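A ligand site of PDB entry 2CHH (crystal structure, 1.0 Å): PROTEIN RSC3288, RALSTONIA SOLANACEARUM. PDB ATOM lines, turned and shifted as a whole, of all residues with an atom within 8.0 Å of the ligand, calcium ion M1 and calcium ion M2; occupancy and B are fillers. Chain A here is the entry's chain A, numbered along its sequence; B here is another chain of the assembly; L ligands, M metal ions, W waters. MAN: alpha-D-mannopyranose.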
ATOM      1  N   ALA A  21      21.735 -33.494 -30.127  1.00  0.00           N
ATOM      2  CA  ALA A  21      21.983 -33.058 -28.757  1.00  0.00           C
ATOM      3  C   ALA A  21      23.438 -33.154 -28.415  1.00  0.00           C
ATOM      4  O   ALA A  21      24.148 -34.071 -28.801  1.00  0.00           O
ATOM      5  CB  ALA A  21      21.177 -33.866 -27.764  1.00  0.00           C
ATOM      6  N   ASN A  22      23.865 -32.189 -27.590  1.00  0.00           N
ATOM      7  CA  ASN A  22      25.148 -32.253 -26.858  1.00  0.00           C
ATOM      8  C   ASN A  22      24.858 -31.738 -25.468  1.00  0.00           C
ATOM      9  O   ASN A  22      25.186 -30.586 -25.123  1.00  0.00           O
ATOM     10  CB  ASN A  22      26.245 -31.427 -27.514  1.00  0.00           C
ATOM     11  CG  ASN A  22      26.636 -31.954 -28.840  1.00  0.00           C
ATOM     12  OD1 ASN A  22      27.455 -32.862 -28.931  1.00  0.00           O
ATOM     13  ND2 ASN A  22      26.063 -31.388 -29.892  1.00  0.00           N
ATOM     14  N   ALA A  23      24.173 -32.519 -24.661  1.00  0.00           N
ATOM     15  CA  ALA A  23      23.551 -32.016 -23.437  1.00  0.00           C
ATOM     16  C   ALA A  23      23.201 -33.169 -22.539  1.00  0.00           C
ATOM     17  O   ALA A  23      22.804 -34.243 -22.993  1.00  0.00           O
ATOM     18  CB  ALA A  23      22.272 -31.268 -23.772  1.00  0.00           C
ATOM     19  N   ALA A  24      23.287 -32.913 -21.226  1.00  0.00           N
ATOM     20  CA  ALA A  24      22.763 -33.867 -20.242  1.00  0.00           C
ATOM     21  C   ALA A  24      21.252 -33.808 -20.170  1.00  0.00           C
ATOM     22  O   ALA A  24      20.586 -34.800 -19.893  1.00  0.00           O
ATOM     23  CB  ALA A  24      23.372 -33.598 -18.898  1.00  0.00           C
ATOM     24  N   ASN A  25      20.663 -32.634 -20.385  1.00  0.00           N
ATOM     25  CA  ASN A  25      19.208 -32.475 -20.310  1.00  0.00           C
ATOM     26  C   ASN A  25      18.549 -32.848 -21.614  1.00  0.00           C
ATOM     27  O   ASN A  25      19.126 -32.659 -22.708  1.00  0.00           O
ATOM     28  CB  ASN A  25      18.849 -31.090 -19.873  1.00  0.00           C
ATOM     29  CG  ASN A  25      19.188 -30.864 -18.363  1.00  0.00           C
ATOM     30  OD1 ASN A  25      19.212 -31.865 -17.603  1.00  0.00           O
ATOM     31  ND2 ASN A  25      19.307 -29.653 -17.944  1.00  0.00           N
ATOM     32  N   THR A  26      17.313 -33.315 -21.521  1.00  0.00           N
ATOM     33  CA  THR A  26      16.553 -33.679 -22.692  1.00  0.00           C
ATOM     34  C   THR A  26      16.158 -32.431 -23.477  1.00  0.00           C
ATOM     35  O   THR A  26      15.489 -31.542 -22.944  1.00  0.00           O
ATOM     36  CB  THR A  26      15.291 -34.429 -22.274  1.00  0.00           C
ATOM     37  OG1 THR A  26      15.687 -35.578 -21.530  1.00  0.00           O
ATOM     38  CG2 THR A  26      14.481 -34.854 -23.463  1.00  0.00           C
ATOM     39  N   GLN A  27      16.558 -32.428 -24.733  1.00  0.00           N
ATOM     40  CA  GLN A  27      16.242 -31.343 -25.650  1.00  0.00           C
ATOM     41  C   GLN A  27      14.946 -31.663 -26.379  1.00  0.00           C
ATOM     42  O   GLN A  27      14.733 -32.791 -26.777  1.00  0.00           O
ATOM     43  CB  GLN A  27      17.362 -31.240 -26.685  1.00  0.00           C
ATOM     44  CG  GLN A  27      18.766 -31.099 -26.064  1.00  0.00           C
ATOM     45  CD  GLN A  27      18.925 -29.832 -25.288  1.00  0.00           C
ATOM     46  OE1 GLN A  27      18.751 -28.759 -25.858  1.00  0.00           O
ATOM     47  NE2 GLN A  27      19.280 -29.929 -24.016  1.00  0.00           N
ATOM     48  N   SER A  44      18.693 -36.618 -25.514  1.00  0.00           N
ATOM     49  CA  SER A  44      19.853 -36.111 -24.795  1.00  0.00           C
ATOM     50  C   SER A  44      21.052 -36.940 -25.164  1.00  0.00           C
ATOM     51  O   SER A  44      20.943 -37.973 -25.811  1.00  0.00           O
ATOM     52  CB  SER A  44      19.648 -36.122 -23.285  1.00  0.00           C
ATOM     53  OG  SER A  44      19.493 -37.443 -22.818  1.00  0.00           O
ATOM     54  N   GLY A  45      22.206 -36.506 -24.713  1.00  0.00           N
ATOM     55  CA  GLY A  45      23.460 -37.193 -24.973  1.00  0.00           C
ATOM     56  C   GLY A  45      24.496 -36.120 -25.262  1.00  0.00           C
ATOM     57  O   GLY A  45      24.186 -35.076 -25.839  1.00  0.00           O
ATOM     58  N   THR A  46      25.725 -36.405 -24.865  1.00  0.00           N
ATOM     59  CA  THR A  46      26.772 -35.378 -24.931  1.00  0.00           C
ATOM     60  C   THR A  46      27.763 -35.555 -26.085  1.00  0.00           C
ATOM     61  O   THR A  46      28.679 -34.760 -26.196  1.00  0.00           O
ATOM     62  CB  THR A  46      27.508 -35.266 -23.608  1.00  0.00           C
ATOM     63  OG1 THR A  46      28.025 -36.555 -23.289  1.00  0.00           O
ATOM     64  CG2 THR A  46      26.568 -34.823 -22.497  1.00  0.00           C
ATOM     65  N   SER A  47      27.546 -36.559 -26.943  1.00  0.00           N
ATOM     66  CA  SER A  47      28.415 -36.867 -28.103  1.00  0.00           C
ATOM     67  C   SER A  47      27.667 -36.724 -29.416  1.00  0.00           C
ATOM     68  O   SER A  47      27.555 -37.654 -30.206  1.00  0.00           O
ATOM     69  CB  SER A  47      29.012 -38.267 -27.974  1.00  0.00           C
ATOM     70  OG  SER A  47      29.938 -38.239 -26.886  1.00  0.00           O
ATOM     71  N   VAL A  69      13.899 -27.114 -23.013  1.00  0.00           N
ATOM     72  CA  VAL A  69      14.179 -28.209 -22.100  1.00  0.00           C
ATOM     73  C   VAL A  69      13.005 -28.193 -21.110  1.00  0.00           C
ATOM     74  O   VAL A  69      12.836 -27.232 -20.350  1.00  0.00           O
ATOM     75  CB  VAL A  69      15.483 -28.056 -21.383  1.00  0.00           C
ATOM     76  CG1 VAL A  69      15.609 -29.159 -20.300  1.00  0.00           C
ATOM     77  CG2 VAL A  69      16.584 -28.121 -22.372  1.00  0.00           C
ATOM     78  N   SER A  94      21.952 -23.750 -29.530  1.00  0.00           N
ATOM     79  CA  SER A  94      21.158 -23.309 -28.381  1.00  0.00           C
ATOM     80  C   SER A  94      21.919 -23.616 -27.104  1.00  0.00           C
ATOM     81  O   SER A  94      22.702 -24.563 -27.028  1.00  0.00           O
ATOM     82  CB  SER A  94      19.815 -23.961 -28.372  1.00  0.00           C
ATOM     83  OG  SER A  94      19.886 -25.374 -28.177  1.00  0.00           O
ATOM     84  N   GLU A  95      21.603 -22.822 -26.091  1.00  0.00           N
ATOM     85  CA  GLU A  95      22.184 -22.938 -24.778  1.00  0.00           C
ATOM     86  C   GLU A  95      21.054 -23.096 -23.764  1.00  0.00           C
ATOM     87  O   GLU A  95      20.172 -22.230 -23.668  1.00  0.00           O
ATOM     88  CB  GLU A  95      23.041 -21.739 -24.436  1.00  0.00           C
ATOM     89  CG  GLU A  95      23.654 -21.796 -23.042  1.00  0.00           C
ATOM     90  CD  GLU A  95      24.443 -23.052 -22.822  1.00  0.00           C
ATOM     91  OE1 GLU A  95      25.287 -23.419 -23.677  1.00  0.00           O
ATOM     92  OE2 GLU A  95      24.209 -23.753 -21.784  1.00  0.00           O
ATOM     93  N   ASP A  96      21.114 -24.184 -22.996  1.00  0.00           N
ATOM     94  CA  ASP A  96      20.114 -24.498 -21.989  1.00  0.00           C
ATOM     95  C   ASP A  96      20.573 -24.194 -20.576  1.00  0.00           C
ATOM     96  O   ASP A  96      19.796 -24.405 -19.628  1.00  0.00           O
ATOM     97  CB  ASP A  96      19.674 -25.965 -22.109  1.00  0.00           C
ATOM     98  CG  ASP A  96      20.735 -26.958 -21.715  1.00  0.00           C
ATOM     99  OD1 ASP A  96      21.739 -26.543 -21.086  1.00  0.00           O
ATOM    100  OD2 ASP A  96      20.561 -28.156 -22.012  1.00  0.00           O
ATOM    101  N   GLY A  97      21.759 -23.655 -20.408  1.00  0.00           N
ATOM    102  CA  GLY A  97      22.384 -23.540 -19.103  1.00  0.00           C
ATOM    103  C   GLY A  97      23.319 -22.395 -19.001  1.00  0.00           C
ATOM    104  O   GLY A  97      22.979 -21.288 -19.425  1.00  0.00           O
ATOM    105  N   THR A  98      24.471 -22.623 -18.402  1.00  0.00           N
ATOM    106  CA  THR A  98      25.410 -21.607 -18.023  1.00  0.00           C
ATOM    107  C   THR A  98      26.783 -21.723 -18.670  1.00  0.00           C
ATOM    108  O   THR A  98      27.557 -20.797 -18.548  1.00  0.00           O
ATOM    109  CB  THR A  98      25.577 -21.565 -16.501  1.00  0.00           C
ATOM    110  OG1 THR A  98      26.049 -22.846 -16.112  1.00  0.00           O
ATOM    111  CG2 THR A  98      24.282 -21.227 -15.789  1.00  0.00           C
ATOM    112  N   ASP A  99      27.108 -22.827 -19.327  1.00  0.00           N
ATOM    113  CA  ASP A  99      28.456 -22.993 -19.845  1.00  0.00           C
ATOM    114  C   ASP A  99      28.657 -22.312 -21.203  1.00  0.00           C
ATOM    115  O   ASP A  99      29.785 -22.178 -21.642  1.00  0.00           O
ATOM    116  CB  ASP A  99      28.901 -24.437 -19.886  1.00  0.00           C
ATOM    117  CG  ASP A  99      28.159 -25.299 -20.865  1.00  0.00           C
ATOM    118  OD1 ASP A  99      27.124 -24.864 -21.407  1.00  0.00           O
ATOM    119  OD2 ASP A  99      28.585 -26.464 -21.057  1.00  0.00           O
ATOM    120  N   ASN A 100      27.589 -21.901 -21.866  1.00  0.00           N
ATOM    121  CA  ASN A 100      27.672 -21.144 -23.115  1.00  0.00           C
ATOM    122  C   ASN A 100      28.455 -21.860 -24.194  1.00  0.00           C
ATOM    123  O   ASN A 100      29.138 -21.232 -25.012  1.00  0.00           O
ATOM    124  CB  ASN A 100      28.186 -19.760 -22.842  1.00  0.00           C
ATOM    125  CG  ASN A 100      27.215 -18.976 -22.026  1.00  0.00           C
ATOM    126  OD1 ASN A 100      26.014 -19.294 -21.936  1.00  0.00           O
ATOM    127  ND2 ASN A 100      27.711 -17.978 -21.346  1.00  0.00           N
ATOM    128  N   ASP A 101      28.209 -23.157 -24.308  1.00  0.00           N
ATOM    129  CA  ASP A 101      28.779 -23.901 -25.426  1.00  0.00           C
ATOM    130  C   ASP A 101      27.835 -23.859 -26.627  1.00  0.00           C
ATOM    131  O   ASP A 101      28.287 -24.119 -27.756  1.00  0.00           O
ATOM    132  CB  ASP A 101      29.205 -25.311 -25.011  1.00  0.00           C
ATOM    133  CG  ASP A 101      28.122 -26.278 -24.547  1.00  0.00           C
ATOM    134  OD1 ASP A 101      26.959 -25.852 -24.397  1.00  0.00           O
ATOM    135  OD2 ASP A 101      28.484 -27.444 -24.320  1.00  0.00           O
ATOM    136  N   TYR A 102      26.566 -23.505 -26.436  1.00  0.00           N
ATOM    137  CA  TYR A 102      25.618 -23.290 -27.538  1.00  0.00           C
ATOM    138  C   TYR A 102      25.442 -24.501 -28.434  1.00  0.00           C
ATOM    139  O   TYR A 102      24.939 -24.384 -29.555  1.00  0.00           O
ATOM    140  CB  TYR A 102      25.926 -22.004 -28.332  1.00  0.00           C
ATOM    141  CG  TYR A 102      25.417 -20.791 -27.568  1.00  0.00           C
ATOM    142  CD1 TYR A 102      26.154 -20.168 -26.604  1.00  0.00           C
ATOM    143  CD2 TYR A 102      24.104 -20.373 -27.725  1.00  0.00           C
ATOM    144  CE1 TYR A 102      25.606 -19.148 -25.845  1.00  0.00           C
ATOM    145  CE2 TYR A 102      23.552 -19.349 -26.958  1.00  0.00           C
ATOM    146  CZ  TYR A 102      24.302 -18.779 -26.013  1.00  0.00           C
ATOM    147  OH  TYR A 102      23.782 -17.793 -25.162  1.00  0.00           O
ATOM    148  N   ASN A 103      25.737 -25.692 -27.917  1.00  0.00           N
ATOM    149  CA  ASN A 103      25.635 -26.907 -28.706  1.00  0.00           C
ATOM    150  C   ASN A 103      24.574 -27.835 -28.171  1.00  0.00           C
ATOM    151  O   ASN A 103      24.490 -29.007 -28.611  1.00  0.00           O
ATOM    152  CB  ASN A 103      26.982 -27.615 -28.803  1.00  0.00           C
ATOM    153  CG  ASN A 103      27.408 -28.175 -27.496  1.00  0.00           C
ATOM    154  OD1 ASN A 103      26.634 -28.122 -26.521  1.00  0.00           O
ATOM    155  ND2 ASN A 103      28.592 -28.758 -27.421  1.00  0.00           N
ATOM    156  N   ASP A 104      23.740 -27.389 -27.233  1.00  0.00           N
ATOM    157  CA  ASP A 104      22.946 -28.318 -26.441  1.00  0.00           C
ATOM    158  C   ASP A 104      21.900 -29.021 -27.284  1.00  0.00           C
ATOM    159  O   ASP A 104      21.722 -30.227 -27.198  1.00  0.00           O
ATOM    160  CB  ASP A 104      22.366 -27.597 -25.245  1.00  0.00           C
ATOM    161  CG  ASP A 104      23.423 -27.036 -24.338  1.00  0.00           C
ATOM    162  OD1 ASP A 104      24.487 -27.678 -24.124  1.00  0.00           O
ATOM    163  OD2 ASP A 104      23.223 -25.920 -23.771  1.00  0.00           O
ATOM    164  N   GLY A 105      21.206 -28.200 -28.093  1.00  0.00           N
ATOM    165  CA  GLY A 105      20.262 -28.654 -29.076  1.00  0.00           C
ATOM    166  C   GLY A 105      20.576 -27.936 -30.371  1.00  0.00           C
ATOM    167  O   GLY A 105      20.601 -26.696 -30.401  1.00  0.00           O
ATOM    168  N   PRO B 112      32.492 -27.593 -30.842  1.00  0.00           N
ATOM    169  CA  PRO B 112      32.767 -28.712 -29.947  1.00  0.00           C
ATOM    170  C   PRO B 112      31.509 -29.445 -29.547  1.00  0.00           C
ATOM    171  O   PRO B 112      30.400 -28.949 -29.653  1.00  0.00           O
ATOM    172  CB  PRO B 112      33.401 -28.045 -28.729  1.00  0.00           C
ATOM    173  CG  PRO B 112      32.725 -26.728 -28.661  1.00  0.00           C
ATOM    174  CD  PRO B 112      32.524 -26.303 -30.125  1.00  0.00           C
ATOM    175  N   LEU B 113      31.724 -30.650 -29.082  1.00  0.00           N
ATOM    176  CA  LEU B 113      30.684 -31.504 -28.517  1.00  0.00           C
ATOM    177  C   LEU B 113      30.633 -31.314 -27.024  1.00  0.00           C
ATOM    178  O   LEU B 113      31.246 -30.398 -26.488  1.00  0.00           O
ATOM    179  CB  LEU B 113      30.887 -32.942 -28.960  1.00  0.00           C
ATOM    180  CG  LEU B 113      31.094 -33.125 -30.463  1.00  0.00           C
ATOM    181  CD1 LEU B 113      31.198 -34.602 -30.789  1.00  0.00           C
ATOM    182  CD2 LEU B 113      30.004 -32.456 -31.282  1.00  0.00           C
ATOM    183  N   GLY B 114      29.901 -32.162 -26.315  1.00  0.00           N
ATOM    184  CA  GLY B 114      29.868 -32.147 -24.851  1.00  0.00           C
ATOM    185  C   GLY B 114      28.697 -31.394 -24.275  1.00  0.00           C
ATOM    186  O   GLY B 114      28.241 -30.391 -24.834  1.00  0.00           O
ATOM    187  OXT GLY B 114      28.280 -31.844 -23.176  1.00  0.00           O
HETATM  188  C1  MAN L   1      26.026 -30.756 -19.976  1.00  0.00           C
HETATM  189  C2  MAN L   1      26.667 -29.880 -21.032  1.00  0.00           C
HETATM  190  C3  MAN L   1      26.133 -28.470 -20.944  1.00  0.00           C
HETATM  191  C4  MAN L   1      24.625 -28.421 -20.916  1.00  0.00           C
HETATM  192  C5  MAN L   1      24.127 -29.269 -19.737  1.00  0.00           C
HETATM  193  C6  MAN L   1      22.658 -29.347 -19.572  1.00  0.00           C
HETATM  194  O1  MAN L   1      26.617 -30.417 -18.746  1.00  0.00           O
HETATM  195  O2  MAN L   1      26.324 -30.377 -22.335  1.00  0.00           O
HETATM  196  O3  MAN L   1      26.621 -27.715 -22.066  1.00  0.00           O
HETATM  197  O4  MAN L   1      24.258 -27.054 -20.798  1.00  0.00           O
HETATM  198  O5  MAN L   1      24.616 -30.621 -19.938  1.00  0.00           O
HETATM  199  O6  MAN L   1      22.024 -29.941 -20.697  1.00  0.00           O
HETATM  200 CA    CA M   1      26.508 -28.837 -24.291  1.00  0.00          CA
HETATM  201 CA    CA M   2      25.335 -25.666 -22.671  1.00  0.00          CA
HETATM  202  O   HOH W   1      25.338 -25.357 -18.670  1.00  0.00           O
HETATM  203  O   HOH W   2      28.307 -28.581 -17.415  1.00  0.00           O
HETATM  204  O   HOH W   3      25.866 -31.665 -16.567  1.00  0.00           O
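An oxygen (O6) of the ligand is in hydrogen-bond range of the side-chain carboxylate (OD2) of Asp 96 (2.7 Å).
N of Ala 24 sits at hydrogen-bond distance from O5 of the ligand.
The backbone NH (N) of Asn 25 lies within hydrogen-bond range of an oxygen (O6) of the ligand (3.0 Å).
The side-chain carboxylate of Asp 104 lies close to the backbone NH of Asp 96, at 2.8 Å.
N of Asp 104 sits at hydrogen-bond distance from O of Ser 94 (3.0 Å).
The backbone carbonyl oxygen of Gly 45 sits close to the backbone NH of Asn 22 (3.4 Å).
The backbone NH of Asn 103 lies within hydrogen-bond range of the backbone carbonyl oxygen of Ser 94, 3.4 Å away.
O of Pro 112 of chain B lies within hydrogen-bond range of ND2 of Asn 103, 2.9 Å away.
The side-chain carboxylate (OE2) of Glu 95 lies close to the backbone NH (N) of Gly 97 (2.8 Å).
The side-chain carboxylate (OE1) of Glu 95 lies close to the backbone NH (N) of Tyr 102 (3.0 Å).
N of Ala 23 sits at hydrogen-bond distance from O of Gly 45.
CB of Ala 23 touches O6 of the ligand, at 3.4 Å.
Within 4 Å of the ligand: Asn 22, Ala 23, Ala 24, Asn 25, Glu 95, Asp 96, Asp 99, Asp 101, Asp 104 and Gly 114 of chain B.
Along chain A the residues within 4 Å of calcium ion M1 span positions 22 to 104.
The nearest printed residue that does not touch calcium ion M1 is Ala 23 (4.4 Å).
Of the 27 residues printed, 4 come within 4 Å of calcium ion M2.
OD1 of Asp 104 is bound to calcium ion M1.
O of Asn 22 is bound to calcium ion M1, 2.3 Å away.
The side-chain amide oxygen (OD1) of Asn 103 is bound to calcium ion M1 (2.3 Å).
Calcium ion M1 is bound by O of Gly 114 of chain B.
Calcium ion M1 is bound by OD2 of Asp 101 (2.4 Å).
Calcium ion M1 is bound by an oxygen (O3) of the ligand (2.5 Å).
Calcium ion M1 is bound by O2 of the ligand.
Slightly farther from calcium ion M1 lies OD1 of Asp 101 (3.0 Å).
The side-chain carboxylate (OD1) of Asp 99 binds calcium ion M2, at 2.3 Å.
Calcium ion M2 is bound by the side-chain carboxylate (OD1) of Asp 101, at 2.4 Å.
OE2 of Glu 95 is bound to calcium ion M2 (2.4 Å).
Calcium ion M2 is bound by the side-chain carboxylate (OD2) of Asp 104, at 2.4 Å.
The side-chain carboxylate (OE1) of Glu 95 binds calcium ion M2 (2.5 Å).
An oxygen (O3) of the ligand is bound to calcium ion M2, 2.5 Å away.
Calcium ion M2 is bound by O4 of the ligand, 2.6 Å away.
Calcium ion M2 is bound by OD1 of Asp 104.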
